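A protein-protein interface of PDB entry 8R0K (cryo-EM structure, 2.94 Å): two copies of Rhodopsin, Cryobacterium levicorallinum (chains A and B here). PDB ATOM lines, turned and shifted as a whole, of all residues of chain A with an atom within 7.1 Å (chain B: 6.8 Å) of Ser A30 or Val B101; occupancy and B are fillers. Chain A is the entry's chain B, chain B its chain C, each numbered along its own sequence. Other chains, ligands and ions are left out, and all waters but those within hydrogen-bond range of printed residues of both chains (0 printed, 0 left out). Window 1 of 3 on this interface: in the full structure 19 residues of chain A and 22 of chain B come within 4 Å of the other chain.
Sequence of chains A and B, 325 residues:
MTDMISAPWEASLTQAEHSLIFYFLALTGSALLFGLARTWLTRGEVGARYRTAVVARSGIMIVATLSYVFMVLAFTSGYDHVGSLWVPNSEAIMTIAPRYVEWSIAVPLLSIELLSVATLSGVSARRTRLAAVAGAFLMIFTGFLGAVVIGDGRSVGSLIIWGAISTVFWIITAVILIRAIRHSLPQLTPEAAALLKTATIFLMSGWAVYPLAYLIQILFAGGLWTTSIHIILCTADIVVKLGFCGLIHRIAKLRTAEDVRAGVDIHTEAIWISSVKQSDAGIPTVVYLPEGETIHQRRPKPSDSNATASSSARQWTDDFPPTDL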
ATOM      1  N   PHE A  22       1.110  13.743 -16.512  1.00  0.00           N
ATOM      2  CA  PHE A  22       2.290  13.404 -17.297  1.00  0.00           C
ATOM      3  C   PHE A  22       3.193  14.616 -17.499  1.00  0.00           C
ATOM      4  O   PHE A  22       4.389  14.535 -17.272  1.00  0.00           O
ATOM      5  CB  PHE A  22       1.914  12.860 -18.670  1.00  0.00           C
ATOM      6  CG  PHE A  22       3.083  12.701 -19.610  1.00  0.00           C
ATOM      7  CD1 PHE A  22       3.460  13.733 -20.466  1.00  0.00           C
ATOM      8  CD2 PHE A  22       3.804  11.509 -19.665  1.00  0.00           C
ATOM      9  CE1 PHE A  22       4.535  13.574 -21.338  1.00  0.00           C
ATOM     10  CE2 PHE A  22       4.881  11.354 -20.540  1.00  0.00           C
ATOM     11  CZ  PHE A  22       5.240  12.387 -21.378  1.00  0.00           C
ATOM     12  N   TYR A  23       2.633  15.745 -17.906  1.00  0.00           N
ATOM     13  CA  TYR A  23       3.429  16.921 -18.173  1.00  0.00           C
ATOM     14  C   TYR A  23       4.302  17.266 -16.984  1.00  0.00           C
ATOM     15  O   TYR A  23       5.460  17.591 -17.180  1.00  0.00           O
ATOM     16  CB  TYR A  23       2.507  18.092 -18.451  1.00  0.00           C
ATOM     17  CG  TYR A  23       3.179  19.438 -18.631  1.00  0.00           C
ATOM     18  CD1 TYR A  23       3.320  20.307 -17.561  1.00  0.00           C
ATOM     19  CD2 TYR A  23       3.594  19.866 -19.884  1.00  0.00           C
ATOM     20  CE1 TYR A  23       3.898  21.550 -17.737  1.00  0.00           C
ATOM     21  CE2 TYR A  23       4.170  21.104 -20.073  1.00  0.00           C
ATOM     22  CZ  TYR A  23       4.327  21.939 -18.991  1.00  0.00           C
ATOM     23  OH  TYR A  23       4.921  23.151 -19.110  1.00  0.00           O
ATOM     24  N   PHE A  24       3.753  17.245 -15.767  1.00  0.00           N
ATOM     25  CA  PHE A  24       4.522  17.629 -14.600  1.00  0.00           C
ATOM     26  C   PHE A  24       5.525  16.539 -14.241  1.00  0.00           C
ATOM     27  O   PHE A  24       6.608  16.850 -13.749  1.00  0.00           O
ATOM     28  CB  PHE A  24       3.618  17.984 -13.446  1.00  0.00           C
ATOM     29  CG  PHE A  24       2.924  19.292 -13.657  1.00  0.00           C
ATOM     30  CD1 PHE A  24       3.520  20.492 -13.343  1.00  0.00           C
ATOM     31  CD2 PHE A  24       1.628  19.325 -14.113  1.00  0.00           C
ATOM     32  CE1 PHE A  24       2.831  21.691 -13.476  1.00  0.00           C
ATOM     33  CE2 PHE A  24       0.941  20.527 -14.249  1.00  0.00           C
ATOM     34  CZ  PHE A  24       1.553  21.712 -13.951  1.00  0.00           C
ATOM     35  N   LEU A  25       5.233  15.275 -14.525  1.00  0.00           N
ATOM     36  CA  LEU A  25       6.236  14.264 -14.255  1.00  0.00           C
ATOM     37  C   LEU A  25       7.369  14.462 -15.237  1.00  0.00           C
ATOM     38  O   LEU A  25       8.521  14.376 -14.849  1.00  0.00           O
ATOM     39  CB  LEU A  25       5.664  12.846 -14.354  1.00  0.00           C
ATOM     40  CG  LEU A  25       4.767  12.428 -13.188  1.00  0.00           C
ATOM     41  CD1 LEU A  25       4.095  11.101 -13.450  1.00  0.00           C
ATOM     42  CD2 LEU A  25       5.541  12.366 -11.884  1.00  0.00           C
ATOM     43  N   ALA A  26       7.061  14.705 -16.496  1.00  0.00           N
ATOM     44  CA  ALA A  26       8.113  14.847 -17.482  1.00  0.00           C
ATOM     45  C   ALA A  26       8.842  16.183 -17.307  1.00  0.00           C
ATOM     46  O   ALA A  26      10.057  16.277 -17.448  1.00  0.00           O
ATOM     47  CB  ALA A  26       7.515  14.715 -18.852  1.00  0.00           C
ATOM     48  N   LEU A  27       8.114  17.234 -17.000  1.00  0.00           N
ATOM     49  CA  LEU A  27       8.752  18.514 -16.798  1.00  0.00           C
ATOM     50  C   LEU A  27       9.732  18.455 -15.617  1.00  0.00           C
ATOM     51  O   LEU A  27      10.807  19.046 -15.683  1.00  0.00           O
ATOM     52  CB  LEU A  27       7.668  19.553 -16.554  1.00  0.00           C
ATOM     53  CG  LEU A  27       8.198  20.958 -16.409  1.00  0.00           C
ATOM     54  CD1 LEU A  27       8.673  21.424 -17.754  1.00  0.00           C
ATOM     55  CD2 LEU A  27       7.116  21.869 -15.874  1.00  0.00           C
ATOM     56  N   THR A  28       9.365  17.790 -14.525  1.00  0.00           N
ATOM     57  CA  THR A  28      10.237  17.738 -13.372  1.00  0.00           C
ATOM     58  C   THR A  28      11.467  16.916 -13.697  1.00  0.00           C
ATOM     59  O   THR A  28      12.570  17.287 -13.383  1.00  0.00           O
ATOM     60  CB  THR A  28       9.533  17.127 -12.166  1.00  0.00           C
ATOM     61  OG1 THR A  28       8.371  17.925 -11.964  1.00  0.00           O
ATOM     62  CG2 THR A  28      10.373  17.106 -10.911  1.00  0.00           C
ATOM     63  N   GLY A  29      11.299  15.793 -14.331  1.00  0.00           N
ATOM     64  CA  GLY A  29      12.456  15.007 -14.660  1.00  0.00           C
ATOM     65  C   GLY A  29      13.370  15.732 -15.636  1.00  0.00           C
ATOM     66  O   GLY A  29      14.575  15.470 -15.633  1.00  0.00           O
ATOM     67  N   SER A  30      12.809  16.592 -16.495  1.00  0.00           N
ATOM     68  CA  SER A  30      13.627  17.301 -17.469  1.00  0.00           C
ATOM     69  C   SER A  30      14.425  18.385 -16.762  1.00  0.00           C
ATOM     70  O   SER A  30      15.628  18.501 -16.944  1.00  0.00           O
ATOM     71  CB  SER A  30      12.801  17.872 -18.586  1.00  0.00           C
ATOM     72  OG  SER A  30      12.174  16.839 -19.336  1.00  0.00           O
ATOM     73  N   ALA A  31      13.737  19.136 -15.915  1.00  0.00           N
ATOM     74  CA  ALA A  31      14.358  20.174 -15.128  1.00  0.00           C
ATOM     75  C   ALA A  31      15.436  19.608 -14.213  1.00  0.00           C
ATOM     76  O   ALA A  31      16.481  20.226 -14.060  1.00  0.00           O
ATOM     77  CB  ALA A  31      13.314  20.880 -14.325  1.00  0.00           C
ATOM     78  N   LEU A  32      15.223  18.457 -13.599  1.00  0.00           N
ATOM     79  CA  LEU A  32      16.265  17.870 -12.778  1.00  0.00           C
ATOM     80  C   LEU A  32      17.443  17.405 -13.618  1.00  0.00           C
ATOM     81  O   LEU A  32      18.562  17.413 -13.119  1.00  0.00           O
ATOM     82  CB  LEU A  32      15.714  16.708 -11.959  1.00  0.00           C
ATOM     83  CG  LEU A  32      14.609  17.140 -10.999  1.00  0.00           C
ATOM     84  CD1 LEU A  32      13.971  15.949 -10.336  1.00  0.00           C
ATOM     85  CD2 LEU A  32      15.102  18.085  -9.942  1.00  0.00           C
ATOM     86  N   LEU A  33      17.219  17.029 -14.868  1.00  0.00           N
ATOM     87  CA  LEU A  33      18.342  16.621 -15.690  1.00  0.00           C
ATOM     88  C   LEU A  33      19.158  17.835 -16.160  1.00  0.00           C
ATOM     89  O   LEU A  33      20.380  17.772 -16.303  1.00  0.00           O
ATOM     90  CB  LEU A  33      17.834  15.783 -16.859  1.00  0.00           C
ATOM     91  CG  LEU A  33      18.949  15.141 -17.655  1.00  0.00           C
ATOM     92  CD1 LEU A  33      19.897  14.345 -16.777  1.00  0.00           C
ATOM     93  CD2 LEU A  33      18.375  14.241 -18.693  1.00  0.00           C
ATOM     94  N   PHE A  34      18.498  18.952 -16.389  1.00  0.00           N
ATOM     95  CA  PHE A  34      19.223  20.168 -16.677  1.00  0.00           C
ATOM     96  C   PHE A  34      20.045  20.579 -15.468  1.00  0.00           C
ATOM     97  O   PHE A  34      21.171  21.030 -15.630  1.00  0.00           O
ATOM     98  CB  PHE A  34      18.250  21.279 -17.017  1.00  0.00           C
ATOM     99  CG  PHE A  34      18.876  22.635 -17.011  1.00  0.00           C
ATOM    100  CD1 PHE A  34      18.480  23.582 -16.088  1.00  0.00           C
ATOM    101  CD2 PHE A  34      19.846  22.960 -17.936  1.00  0.00           C
ATOM    102  CE1 PHE A  34      19.033  24.853 -16.108  1.00  0.00           C
ATOM    103  CE2 PHE A  34      20.373  24.236 -17.975  1.00  0.00           C
ATOM    104  CZ  PHE A  34      19.971  25.177 -17.055  1.00  0.00           C
ATOM    105  N   GLY A  35      19.456  20.437 -14.277  1.00  0.00           N
ATOM    106  CA  GLY A  35      20.124  20.716 -13.020  1.00  0.00           C
ATOM    107  C   GLY A  35      21.383  19.876 -12.840  1.00  0.00           C
ATOM    108  O   GLY A  35      22.351  20.343 -12.248  1.00  0.00           O
ATOM    109  N   LEU A  36      21.362  18.646 -13.338  1.00  0.00           N
ATOM    110  CA  LEU A  36      22.526  17.797 -13.259  1.00  0.00           C
ATOM    111  C   LEU A  36      23.583  18.358 -14.201  1.00  0.00           C
ATOM    112  O   LEU A  36      24.743  18.504 -13.811  1.00  0.00           O
ATOM    113  CB  LEU A  36      22.129  16.359 -13.596  1.00  0.00           C
ATOM    114  CG  LEU A  36      23.233  15.321 -13.436  1.00  0.00           C
ATOM    115  CD1 LEU A  36      23.860  15.359 -12.045  1.00  0.00           C
ATOM    116  CD2 LEU A  36      22.702  13.942 -13.696  1.00  0.00           C
ATOM    117  N   THR A  65      16.585  12.558 -10.800  1.00  0.00           N
ATOM    118  CA  THR A  65      16.345  12.424 -12.219  1.00  0.00           C
ATOM    119  C   THR A  65      15.931  11.007 -12.518  1.00  0.00           C
ATOM    120  O   THR A  65      15.105  10.820 -13.408  1.00  0.00           O
ATOM    121  CB  THR A  65      17.563  12.767 -13.082  1.00  0.00           C
ATOM    122  OG1 THR A  65      17.864  14.156 -12.897  1.00  0.00           O
ATOM    123  CG2 THR A  65      17.325  12.532 -14.554  1.00  0.00           C
ATOM    124  N   TYR A  68      12.306  10.300 -11.385  1.00  0.00           N
ATOM    125  CA  TYR A  68      11.260  10.868 -12.204  1.00  0.00           C
ATOM    126  C   TYR A  68      11.225  10.211 -13.562  1.00  0.00           C
ATOM    127  O   TYR A  68      10.222  10.319 -14.250  1.00  0.00           O
ATOM    128  CB  TYR A  68      11.375  12.370 -12.385  1.00  0.00           C
ATOM    129  CG  TYR A  68      10.690  13.081 -11.232  1.00  0.00           C
ATOM    130  CD1 TYR A  68       9.376  13.517 -11.360  1.00  0.00           C
ATOM    131  CD2 TYR A  68      11.325  13.263 -10.018  1.00  0.00           C
ATOM    132  CE1 TYR A  68       8.723  14.155 -10.325  1.00  0.00           C
ATOM    133  CE2 TYR A  68      10.689  13.917  -8.986  1.00  0.00           C
ATOM    134  CZ  TYR A  68       9.382  14.359  -9.132  1.00  0.00           C
ATOM    135  OH  TYR A  68       8.669  15.006  -8.149  1.00  0.00           O
ATOM    136  N   VAL A  69      12.301   9.538 -13.940  1.00  0.00           N
ATOM    137  CA  VAL A  69      12.264   8.736 -15.144  1.00  0.00           C
ATOM    138  C   VAL A  69      11.443   7.477 -14.880  1.00  0.00           C
ATOM    139  O   VAL A  69      10.590   7.085 -15.662  1.00  0.00           O
ATOM    140  CB  VAL A  69      13.685   8.417 -15.614  1.00  0.00           C
ATOM    141  CG1 VAL A  69      13.694   7.370 -16.727  1.00  0.00           C
ATOM    142  CG2 VAL A  69      14.360   9.707 -16.050  1.00  0.00           C
ATOM    143  N   LEU A 242      16.094  22.880  -7.568  1.00  0.00           N
ATOM    144  CA  LEU A 242      16.875  23.722  -8.465  1.00  0.00           C
ATOM    145  C   LEU A 242      17.205  25.061  -7.840  1.00  0.00           C
ATOM    146  O   LEU A 242      18.279  25.593  -8.096  1.00  0.00           O
ATOM    147  CB  LEU A 242      16.143  23.958  -9.781  1.00  0.00           C
ATOM    148  CG  LEU A 242      15.972  22.714 -10.640  1.00  0.00           C
ATOM    149  CD1 LEU A 242      15.204  23.074 -11.879  1.00  0.00           C
ATOM    150  CD2 LEU A 242      17.301  22.068 -11.023  1.00  0.00           C
ATOM    151  N   GLY B  59      21.531  22.391 -21.664  1.00  0.00           N
ATOM    152  CA  GLY B  59      20.191  22.106 -21.190  1.00  0.00           C
ATOM    153  C   GLY B  59      19.182  21.987 -22.315  1.00  0.00           C
ATOM    154  O   GLY B  59      18.363  21.093 -22.280  1.00  0.00           O
ATOM    155  N   ILE B  62      19.879  18.666 -24.076  1.00  0.00           N
ATOM    156  CA  ILE B  62      19.657  17.441 -23.345  1.00  0.00           C
ATOM    157  C   ILE B  62      18.157  17.200 -23.244  1.00  0.00           C
ATOM    158  O   ILE B  62      17.694  16.089 -23.467  1.00  0.00           O
ATOM    159  CB  ILE B  62      20.294  17.488 -21.952  1.00  0.00           C
ATOM    160  CG1 ILE B  62      21.801  17.679 -22.015  1.00  0.00           C
ATOM    161  CG2 ILE B  62      19.973  16.221 -21.181  1.00  0.00           C
ATOM    162  CD1 ILE B  62      22.415  17.972 -20.672  1.00  0.00           C
ATOM    163  N   VAL B  63      17.400  18.230 -22.907  1.00  0.00           N
ATOM    164  CA  VAL B  63      15.975  18.097 -22.758  1.00  0.00           C
ATOM    165  C   VAL B  63      15.377  17.714 -24.102  1.00  0.00           C
ATOM    166  O   VAL B  63      14.572  16.783 -24.175  1.00  0.00           O
ATOM    167  CB  VAL B  63      15.377  19.397 -22.226  1.00  0.00           C
ATOM    168  CG1 VAL B  63      13.863  19.340 -22.208  1.00  0.00           C
ATOM    169  CG2 VAL B  63      15.904  19.694 -20.837  1.00  0.00           C
ATOM    170  N   LEU B  66      15.958  14.096 -25.198  1.00  0.00           N
ATOM    171  CA  LEU B  66      15.171  13.090 -24.492  1.00  0.00           C
ATOM    172  C   LEU B  66      13.722  13.124 -24.953  1.00  0.00           C
ATOM    173  O   LEU B  66      13.100  12.085 -25.165  1.00  0.00           O
ATOM    174  CB  LEU B  66      15.239  13.326 -22.993  1.00  0.00           C
ATOM    175  CG  LEU B  66      16.614  13.076 -22.409  1.00  0.00           C
ATOM    176  CD1 LEU B  66      16.498  13.107 -20.901  1.00  0.00           C
ATOM    177  CD2 LEU B  66      17.224  11.774 -22.948  1.00  0.00           C
ATOM    178  N   SER B  67      13.202  14.328 -25.120  1.00  0.00           N
ATOM    179  CA  SER B  67      11.864  14.453 -25.623  1.00  0.00           C
ATOM    180  C   SER B  67      11.724  13.672 -26.930  1.00  0.00           C
ATOM    181  O   SER B  67      10.757  12.940 -27.105  1.00  0.00           O
ATOM    182  CB  SER B  67      11.518  15.912 -25.757  1.00  0.00           C
ATOM    183  OG  SER B  67      10.187  16.081 -26.239  1.00  0.00           O
ATOM    184  N   ILE B  96       2.946  13.685 -29.452  1.00  0.00           N
ATOM    185  CA  ILE B  96       2.910  15.108 -29.739  1.00  0.00           C
ATOM    186  C   ILE B  96       2.977  15.888 -28.430  1.00  0.00           C
ATOM    187  O   ILE B  96       3.492  16.998 -28.405  1.00  0.00           O
ATOM    188  CB  ILE B  96       1.688  15.513 -30.599  1.00  0.00           C
ATOM    189  CG1 ILE B  96       0.389  15.450 -29.804  1.00  0.00           C
ATOM    190  CG2 ILE B  96       1.581  14.707 -31.886  1.00  0.00           C
ATOM    191  CD1 ILE B  96       0.176  16.643 -28.898  1.00  0.00           C
ATOM    192  N   ALA B  97       2.448  15.324 -27.351  1.00  0.00           N
ATOM    193  CA  ALA B  97       2.389  16.032 -26.085  1.00  0.00           C
ATOM    194  C   ALA B  97       3.755  16.249 -25.448  1.00  0.00           C
ATOM    195  O   ALA B  97       3.905  17.247 -24.767  1.00  0.00           O
ATOM    196  CB  ALA B  97       1.505  15.286 -25.127  1.00  0.00           C
ATOM    197  N   PRO B  98       4.753  15.341 -25.578  1.00  0.00           N
ATOM    198  CA  PRO B  98       6.110  15.553 -25.052  1.00  0.00           C
ATOM    199  C   PRO B  98       6.836  16.808 -25.534  1.00  0.00           C
ATOM    200  O   PRO B  98       7.671  17.331 -24.803  1.00  0.00           O
ATOM    201  CB  PRO B  98       6.918  14.348 -25.528  1.00  0.00           C
ATOM    202  CG  PRO B  98       5.834  13.316 -25.615  1.00  0.00           C
ATOM    203  CD  PRO B  98       4.651  14.038 -26.225  1.00  0.00           C
ATOM    204  N   ARG B  99       6.486  17.308 -26.724  1.00  0.00           N
ATOM    205  CA  ARG B  99       7.069  18.537 -27.193  1.00  0.00           C
ATOM    206  C   ARG B  99       6.818  19.677 -26.213  1.00  0.00           C
ATOM    207  O   ARG B  99       7.667  20.536 -26.014  1.00  0.00           O
ATOM    208  CB  ARG B  99       6.525  18.917 -28.558  1.00  0.00           C
ATOM    209  CG  ARG B  99       7.215  18.184 -29.694  1.00  0.00           C
ATOM    210  CD  ARG B  99       7.011  18.822 -31.070  1.00  0.00           C
ATOM    211  NE  ARG B  99       7.562  18.002 -32.150  1.00  0.00           N
ATOM    212  CZ  ARG B  99       6.847  17.132 -32.848  1.00  0.00           C
ATOM    213  NH1 ARG B  99       7.342  16.625 -33.953  1.00  0.00           N
ATOM    214  NH2 ARG B  99       5.619  16.798 -32.483  1.00  0.00           N
ATOM    215  N   TYR B 100       5.656  19.730 -25.602  1.00  0.00           N
ATOM    216  CA  TYR B 100       5.343  20.849 -24.732  1.00  0.00           C
ATOM    217  C   TYR B 100       6.198  20.766 -23.483  1.00  0.00           C
ATOM    218  O   TYR B 100       6.528  21.797 -22.914  1.00  0.00           O
ATOM    219  CB  TYR B 100       3.852  20.834 -24.370  1.00  0.00           C
ATOM    220  CG  TYR B 100       2.978  21.262 -25.542  1.00  0.00           C
ATOM    221  CD1 TYR B 100       2.762  22.605 -25.799  1.00  0.00           C
ATOM    222  CD2 TYR B 100       2.489  20.344 -26.450  1.00  0.00           C
ATOM    223  CE1 TYR B 100       2.035  23.028 -26.890  1.00  0.00           C
ATOM    224  CE2 TYR B 100       1.786  20.757 -27.563  1.00  0.00           C
ATOM    225  CZ  TYR B 100       1.539  22.104 -27.774  1.00  0.00           C
ATOM    226  OH  TYR B 100       0.834  22.663 -28.811  1.00  0.00           O
ATOM    227  N   VAL B 101       6.557  19.553 -23.058  1.00  0.00           N
ATOM    228  CA  VAL B 101       7.467  19.404 -21.941  1.00  0.00           C
ATOM    229  C   VAL B 101       8.838  19.971 -22.311  1.00  0.00           C
ATOM    230  O   VAL B 101       9.409  20.761 -21.555  1.00  0.00           O
ATOM    231  CB  VAL B 101       7.546  17.939 -21.514  1.00  0.00           C
ATOM    232  CG1 VAL B 101       8.567  17.712 -20.422  1.00  0.00           C
ATOM    233  CG2 VAL B 101       6.199  17.490 -21.027  1.00  0.00           C
ATOM    234  N   GLU B 102       9.345  19.586 -23.485  1.00  0.00           N
ATOM    235  CA  GLU B 102      10.590  20.117 -24.005  1.00  0.00           C
ATOM    236  C   GLU B 102      10.539  21.628 -24.131  1.00  0.00           C
ATOM    237  O   GLU B 102      11.429  22.281 -23.631  1.00  0.00           O
ATOM    238  CB  GLU B 102      10.894  19.542 -25.370  1.00  0.00           C
ATOM    239  CG  GLU B 102      11.718  20.471 -26.233  1.00  0.00           C
ATOM    240  CD  GLU B 102      11.705  20.106 -27.706  1.00  0.00           C
ATOM    241  OE1 GLU B 102      12.190  20.915 -28.519  1.00  0.00           O
ATOM    242  OE2 GLU B 102      11.215  19.003 -28.040  1.00  0.00           O
ATOM    243  N   TRP B 103       9.532  22.186 -24.791  1.00  0.00           N
ATOM    244  CA  TRP B 103       9.472  23.630 -24.991  1.00  0.00           C
ATOM    245  C   TRP B 103       9.376  24.375 -23.676  1.00  0.00           C
ATOM    246  O   TRP B 103       9.836  25.491 -23.579  1.00  0.00           O
ATOM    247  CB  TRP B 103       8.306  24.054 -25.887  1.00  0.00           C
ATOM    248  CG  TRP B 103       8.398  23.535 -27.292  1.00  0.00           C
ATOM    249  CD1 TRP B 103       9.494  23.069 -27.960  1.00  0.00           C
ATOM    250  CD2 TRP B 103       7.291  23.360 -28.189  1.00  0.00           C
ATOM    251  NE1 TRP B 103       9.165  22.681 -29.228  1.00  0.00           N
ATOM    252  CE2 TRP B 103       7.812  22.838 -29.387  1.00  0.00           C
ATOM    253  CE3 TRP B 103       5.915  23.586 -28.092  1.00  0.00           C
ATOM    254  CZ2 TRP B 103       6.987  22.540 -30.466  1.00  0.00           C
ATOM    255  CZ3 TRP B 103       5.114  23.294 -29.167  1.00  0.00           C
ATOM    256  CH2 TRP B 103       5.644  22.783 -30.335  1.00  0.00           C
ATOM    257  N   SER B 104       8.796  23.772 -22.662  1.00  0.00           N
ATOM    258  CA  SER B 104       8.646  24.476 -21.406  1.00  0.00           C
ATOM    259  C   SER B 104       9.996  24.805 -20.779  1.00  0.00           C
ATOM    260  O   SER B 104      10.080  25.773 -20.038  1.00  0.00           O
ATOM    261  CB  SER B 104       7.817  23.683 -20.458  1.00  0.00           C
ATOM    262  OG  SER B 104       6.512  23.573 -20.976  1.00  0.00           O
ATOM    263  N   ILE B 105      11.010  23.971 -21.029  1.00  0.00           N
ATOM    264  CA  ILE B 105      12.325  24.110 -20.431  1.00  0.00           C
ATOM    265  C   ILE B 105      13.228  24.854 -21.412  1.00  0.00           C
ATOM    266  O   ILE B 105      14.205  25.453 -21.005  1.00  0.00           O
ATOM    267  CB  ILE B 105      12.848  22.706 -20.059  1.00  0.00           C
ATOM    268  CG1 ILE B 105      11.921  22.034 -19.060  1.00  0.00           C
ATOM    269  CG2 ILE B 105      14.238  22.747 -19.485  1.00  0.00           C
ATOM    270  CD1 ILE B 105      11.755  22.860 -17.791  1.00  0.00           C
ATOM    271  N   ALA B 106      12.902  24.847 -22.697  1.00  0.00           N
ATOM    272  CA  ALA B 106      13.860  25.215 -23.716  1.00  0.00           C
ATOM    273  C   ALA B 106      13.556  26.599 -24.239  1.00  0.00           C
ATOM    274  O   ALA B 106      14.468  27.270 -24.690  1.00  0.00           O
ATOM    275  CB  ALA B 106      13.857  24.215 -24.836  1.00  0.00           C
ATOM    276  N   ILE B 140       4.196  28.689 -23.189  1.00  0.00           N
ATOM    277  CA  ILE B 140       4.187  27.289 -23.526  1.00  0.00           C
ATOM    278  C   ILE B 140       3.107  26.559 -22.748  1.00  0.00           C
ATOM    279  O   ILE B 140       2.409  25.743 -23.341  1.00  0.00           O
ATOM    280  CB  ILE B 140       5.580  26.701 -23.291  1.00  0.00           C
ATOM    281  CG1 ILE B 140       6.602  27.429 -24.169  1.00  0.00           C
ATOM    282  CG2 ILE B 140       5.553  25.197 -23.531  1.00  0.00           C
ATOM    283  CD1 ILE B 140       6.277  27.387 -25.649  1.00  0.00           C
ATOM    284  N   PHE B 144      -0.156  24.477 -23.980  1.00  0.00           N
ATOM    285  CA  PHE B 144      -0.332  23.077 -23.682  1.00  0.00           C
ATOM    286  C   PHE B 144      -1.741  22.818 -23.178  1.00  0.00           C
ATOM    287  O   PHE B 144      -2.306  21.776 -23.491  1.00  0.00           O
ATOM    288  CB  PHE B 144       0.670  22.652 -22.622  1.00  0.00           C
ATOM    289  CG  PHE B 144       0.472  21.263 -22.066  1.00  0.00           C
ATOM    290  CD1 PHE B 144       0.144  21.080 -20.738  1.00  0.00           C
ATOM    291  CD2 PHE B 144       0.661  20.151 -22.867  1.00  0.00           C
ATOM    292  CE1 PHE B 144      -0.014  19.813 -20.225  1.00  0.00           C
ATOM    293  CE2 PHE B 144       0.459  18.886 -22.356  1.00  0.00           C
ATOM    294  CZ  PHE B 144       0.125  18.722 -21.037  1.00  0.00           C
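The side-chain hydroxyl (OH) of Tyr A23 lies within hydrogen-bond range of the side-chain hydroxyl (OG) of Ser B104 (2.5 Å).
OG of Ser A30 is in hydrogen-bond range of O of Ala A26 (2.9 Å).
The backbone carbonyl oxygen (O) of Tyr B100 lies within hydrogen-bond range of the side-chain hydroxyl (OG) of Ser B104.
Among the printed residues, merely in contact across the chains: Tyr A23 with Tyr B100 (3.8 Å), Tyr A23 with Val B101 (3.7 Å), Tyr A23 with Phe B144 (3.5 Å), Ala A26 with Val B101 (3.5 Å), Leu A27 with Val B101 (3.5 Å), Leu A27 with Ser B104 (3.6 Å), Leu A27 with Ile B105 (3.4 Å), Ser A30 with Val B101 (3.9 Å), Leu A33 with Ile B62 (3.6 Å), Leu A33 with Leu B66 (3.1 Å) and Phe A34 with Gly B59 (3.4 Å).
Ser A30 touches just one residue of chain B: Val B101.
Val B101 touches just these residues of chain A: Tyr A23, Ala A26, Leu A27 and Ser A30.
Printed residues of chain B within 4 Å of Phe A34: Gly B59.
Printed residues of chain A within 4 Å of Tyr B100: Tyr A23 (3.8 Å).
Of the 18 printed residues of chain B, 8 touch a printed residue of chain A.
Printed residues of chain B that touch a printed residue of chain A: Gly B59, Ile B62, Leu B66, Tyr B100, Val B101, Ser B104, Ile B105 and Phe B144.
Hydrophobic or aromatic side chains of chain B within 4 Å of the printed part of chain A: Ile B62, Leu B66, Val B101, Ile B105 and Phe B144.
Of the 19 printed residues of chain A, 6 touch a printed residue of chain B.
Among the printed residues, 12 pairs touch across the chains.
Among the printed residues, no Asp or Glu carboxylate lies within 4 Å of a Lys or Arg side-chain nitrogen of the other chain.
No position is printed for both chains.
Of the 12 pairs that touch across the chains among the printed residues, none has its exchanged pair printed and touching as well.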
